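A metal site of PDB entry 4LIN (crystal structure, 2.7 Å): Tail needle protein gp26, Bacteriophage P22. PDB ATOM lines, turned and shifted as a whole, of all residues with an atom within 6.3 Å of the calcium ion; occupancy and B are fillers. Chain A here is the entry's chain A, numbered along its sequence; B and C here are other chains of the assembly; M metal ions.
The side-chain amide oxygen (OD1) of Asn 74 of chain B sits at hydrogen-bond distance from the side-chain amide nitrogen (ND2) of Asn 74 of chain A (3.4 Å). The backbone carbonyl oxygen (O) of Ala 70 of chain A sits close to the side-chain amide nitrogen (ND2) of Asn 74 of chain A, 3.4 Å away. The side-chain amide nitrogen (NE2) of Gln 77 of chain C lies close to the side-chain amide oxygen (OE1) of Gln 77 of chain A (2.4 Å). NE2 of Gln 77 of chain C sits close to OD1 of Asn 74 of chain C, at 2.5 Å. ND2 of Asn 74 of chain C lies within hydrogen-bond range of O of Ala 70 of chain C (2.5 Å). The side-chain amide oxygen (OE1) of Gln 77 of chain C lies close to the backbone carbonyl oxygen (O) of Asn 74 of chain B, at 3.1 Å. OD1 of Asn 74 of chain B sits close to O of Ala 70 of chain B (2.8 Å). The side-chain amide nitrogen (ND2) of Asn 74 of chain B is in hydrogen-bond range of the backbone carbonyl oxygen (O) of Ala 70 of chain C (3.2 Å).
Lys 73 of chain A touches the calcium ion (O to CA, 3.7 Å). Asn 74 of chain B touches the calcium ion. Of the 14 residues printed, 7 come within 4 Å of the calcium ion. The nearest printed residue that does not touch the calcium ion is Asp 78 (4.3 Å).
The calcium ion is bound by the side-chain amide oxygen (OD1) of Asn 74 of chain A (2.3 Å). OE1 of Gln 77 of chain B is bound to the calcium ion, 2.4 Å away. The calcium ion is bound by the side-chain amide oxygen (OE1) of Gln 77 of chain A, at 2.4 Å. OD1 of Asn 74 of chain C is bound to the calcium ion, 2.5 Å away. The calcium ion is bound by NE2 of Gln 77 of chain B (2.5 Å). Slightly farther from the calcium ion lies the side-chain amide nitrogen (NE2) of Gln 77 of chain C (3.1 Å).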
ATOM      1  N   ALA A  70     -22.330  20.109  15.295  1.00  0.00           N
ATOM      2  CA  ALA A  70     -21.143  19.790  16.076  1.00  0.00           C
ATOM      3  C   ALA A  70     -19.854  20.126  15.325  1.00  0.00           C
ATOM      4  O   ALA A  70     -18.770  20.163  15.928  1.00  0.00           O
ATOM      5  CB  ALA A  70     -21.135  18.331  16.493  1.00  0.00           C
ATOM      6  N   LYS A  73     -19.498  24.191  15.972  1.00  0.00           N
ATOM      7  CA  LYS A  73     -18.985  24.483  17.306  1.00  0.00           C
ATOM      8  C   LYS A  73     -17.575  23.950  17.473  1.00  0.00           C
ATOM      9  O   LYS A  73     -16.846  24.372  18.369  1.00  0.00           O
ATOM     10  CB  LYS A  73     -19.912  23.926  18.388  1.00  0.00           C
ATOM     11  CG  LYS A  73     -20.061  22.413  18.385  1.00  0.00           C
ATOM     12  CD  LYS A  73     -20.994  21.936  19.494  1.00  0.00           C
ATOM     13  CE  LYS A  73     -22.353  22.605  19.401  1.00  0.00           C
ATOM     14  NZ  LYS A  73     -23.284  22.171  20.476  1.00  0.00           N
ATOM     15  N   ASN A  74     -17.183  23.021  16.607  1.00  0.00           N
ATOM     16  CA  ASN A  74     -15.818  22.510  16.582  1.00  0.00           C
ATOM     17  C   ASN A  74     -14.883  23.545  15.969  1.00  0.00           C
ATOM     18  O   ASN A  74     -13.998  24.069  16.643  1.00  0.00           O
ATOM     19  CB  ASN A  74     -15.723  21.217  15.775  1.00  0.00           C
ATOM     20  CG  ASN A  74     -15.895  19.970  16.630  1.00  0.00           C
ATOM     21  OD1 ASN A  74     -16.292  20.050  17.787  1.00  0.00           O
ATOM     22  ND2 ASN A  74     -15.605  18.808  16.046  1.00  0.00           N
ATOM     23  N   ASP A  75     -15.093  23.846  14.689  1.00  0.00           N
ATOM     24  CA  ASP A  75     -14.239  24.773  13.955  1.00  0.00           C
ATOM     25  C   ASP A  75     -14.185  26.166  14.582  1.00  0.00           C
ATOM     26  O   ASP A  75     -13.270  26.945  14.310  1.00  0.00           O
ATOM     27  CB  ASP A  75     -14.690  24.861  12.486  1.00  0.00           C
ATOM     28  CG  ASP A  75     -14.524  23.544  11.746  1.00  0.00           C
ATOM     29  OD1 ASP A  75     -13.976  22.597  12.340  1.00  0.00           O
ATOM     30  OD2 ASP A  75     -14.934  23.469  10.571  1.00  0.00           O
ATOM     31  N   GLU A  76     -15.173  26.488  15.412  1.00  0.00           N
ATOM     32  CA  GLU A  76     -15.176  27.741  16.164  1.00  0.00           C
ATOM     33  C   GLU A  76     -14.263  27.656  17.381  1.00  0.00           C
ATOM     34  O   GLU A  76     -13.705  28.657  17.823  1.00  0.00           O
ATOM     35  CB  GLU A  76     -16.595  28.115  16.605  1.00  0.00           C
ATOM     36  CG  GLU A  76     -17.304  29.074  15.666  1.00  0.00           C
ATOM     37  CD  GLU A  76     -18.648  29.532  16.199  1.00  0.00           C
ATOM     38  OE1 GLU A  76     -18.928  29.278  17.400  1.00  0.00           O
ATOM     39  OE2 GLU A  76     -19.420  30.134  15.440  1.00  0.00           O
ATOM     40  N   GLN A  77     -14.106  26.452  17.932  1.00  0.00           N
ATOM     41  CA  GLN A  77     -13.223  26.241  19.070  1.00  0.00           C
ATOM     42  C   GLN A  77     -11.766  26.166  18.622  1.00  0.00           C
ATOM     43  O   GLN A  77     -10.861  26.573  19.353  1.00  0.00           O
ATOM     44  CB  GLN A  77     -13.594  24.960  19.810  1.00  0.00           C
ATOM     45  CG  GLN A  77     -14.853  25.062  20.668  1.00  0.00           C
ATOM     46  CD  GLN A  77     -15.263  23.723  21.237  1.00  0.00           C
ATOM     47  OE1 GLN A  77     -14.668  22.696  20.922  1.00  0.00           O
ATOM     48  NE2 GLN A  77     -16.292  23.725  22.079  1.00  0.00           N
ATOM     49  N   ASP A  78     -11.553  25.644  17.413  1.00  0.00           N
ATOM     50  CA  ASP A  78     -10.209  25.418  16.898  1.00  0.00           C
ATOM     51  C   ASP A  78      -9.405  26.711  16.694  1.00  0.00           C
ATOM     52  O   ASP A  78      -8.180  26.710  16.842  1.00  0.00           O
ATOM     53  CB  ASP A  78     -10.272  24.599  15.611  1.00  0.00           C
ATOM     54  CG  ASP A  78     -10.785  23.199  15.846  1.00  0.00           C
ATOM     55  OD1 ASP A  78     -11.400  22.966  16.903  1.00  0.00           O
ATOM     56  OD2 ASP A  78     -10.558  22.320  14.985  1.00  0.00           O
ATOM     57  N   ALA B  70     -16.530  14.460  14.053  1.00  0.00           N
ATOM     58  CA  ALA B  70     -16.750  15.412  15.128  1.00  0.00           C
ATOM     59  C   ALA B  70     -16.269  14.825  16.460  1.00  0.00           C
ATOM     60  O   ALA B  70     -15.864  15.552  17.360  1.00  0.00           O
ATOM     61  CB  ALA B  70     -18.201  15.833  15.204  1.00  0.00           C
ATOM     62  N   LYS B  73     -12.357  14.778  16.323  1.00  0.00           N
ATOM     63  CA  LYS B  73     -11.854  16.136  16.469  1.00  0.00           C
ATOM     64  C   LYS B  73     -11.837  16.501  17.955  1.00  0.00           C
ATOM     65  O   LYS B  73     -10.883  17.114  18.444  1.00  0.00           O
ATOM     66  CB  LYS B  73     -12.714  17.131  15.687  1.00  0.00           C
ATOM     67  CG  LYS B  73     -11.951  18.348  15.182  1.00  0.00           C
ATOM     68  CD  LYS B  73     -10.781  17.928  14.319  1.00  0.00           C
ATOM     69  CE  LYS B  73     -10.089  19.125  13.659  1.00  0.00           C
ATOM     70  NZ  LYS B  73      -9.558  20.107  14.648  1.00  0.00           N
ATOM     71  N   ASN B  74     -12.895  16.114  18.644  1.00  0.00           N
ATOM     72  CA  ASN B  74     -13.021  16.351  20.078  1.00  0.00           C
ATOM     73  C   ASN B  74     -11.901  15.676  20.871  1.00  0.00           C
ATOM     74  O   ASN B  74     -11.567  16.109  21.970  1.00  0.00           O
ATOM     75  CB  ASN B  74     -14.394  15.866  20.582  1.00  0.00           C
ATOM     76  CG  ASN B  74     -15.534  16.756  20.130  1.00  0.00           C
ATOM     77  OD1 ASN B  74     -15.401  17.550  19.201  1.00  0.00           O
ATOM     78  ND2 ASN B  74     -16.680  16.624  20.795  1.00  0.00           N
ATOM     79  N   GLN B  77      -8.862  17.770  20.352  1.00  0.00           N
ATOM     80  CA  GLN B  77      -9.084  18.995  21.098  1.00  0.00           C
ATOM     81  C   GLN B  77      -8.767  18.819  22.576  1.00  0.00           C
ATOM     82  O   GLN B  77      -8.128  19.669  23.186  1.00  0.00           O
ATOM     83  CB  GLN B  77     -10.513  19.508  20.898  1.00  0.00           C
ATOM     84  CG  GLN B  77     -10.734  20.123  19.520  1.00  0.00           C
ATOM     85  CD  GLN B  77     -12.169  20.554  19.301  1.00  0.00           C
ATOM     86  OE1 GLN B  77     -13.069  20.124  20.013  1.00  0.00           O
ATOM     87  NE2 GLN B  77     -12.371  21.416  18.317  1.00  0.00           N
ATOM     88  N   ALA C  70     -20.730  14.128  20.301  1.00  0.00           N
ATOM     89  CA  ALA C  70     -19.776  15.053  19.732  1.00  0.00           C
ATOM     90  C   ALA C  70     -20.213  16.479  20.063  1.00  0.00           C
ATOM     91  O   ALA C  70     -19.589  17.449  19.636  1.00  0.00           O
ATOM     92  CB  ALA C  70     -19.684  14.865  18.239  1.00  0.00           C
ATOM     93  N   ASN C  74     -18.137  18.769  23.408  1.00  0.00           N
ATOM     94  CA  ASN C  74     -17.888  20.164  23.048  1.00  0.00           C
ATOM     95  C   ASN C  74     -18.413  21.126  24.108  1.00  0.00           C
ATOM     96  O   ASN C  74     -17.909  22.245  24.248  1.00  0.00           O
ATOM     97  CB  ASN C  74     -18.475  20.486  21.678  1.00  0.00           C
ATOM     98  CG  ASN C  74     -17.560  20.102  20.541  1.00  0.00           C
ATOM     99  OD1 ASN C  74     -16.352  20.333  20.597  1.00  0.00           O
ATOM    100  ND2 ASN C  74     -18.124  19.503  19.493  1.00  0.00           N
ATOM    101  N   GLN C  77     -15.931  21.038  26.559  1.00  0.00           N
ATOM    102  CA  GLN C  77     -14.799  21.727  25.949  1.00  0.00           C
ATOM    103  C   GLN C  77     -14.923  23.241  26.113  1.00  0.00           C
ATOM    104  O   GLN C  77     -13.920  23.934  26.187  1.00  0.00           O
ATOM    105  CB  GLN C  77     -14.647  21.350  24.486  1.00  0.00           C
ATOM    106  CG  GLN C  77     -14.012  19.987  24.279  1.00  0.00           C
ATOM    107  CD  GLN C  77     -13.783  19.686  22.823  1.00  0.00           C
ATOM    108  OE1 GLN C  77     -13.153  18.687  22.479  1.00  0.00           O
ATOM    109  NE2 GLN C  77     -14.299  20.546  21.954  1.00  0.00           N
HETATM  110 CA    CA M   1     -14.815  21.346  18.971  1.00  0.00          CA
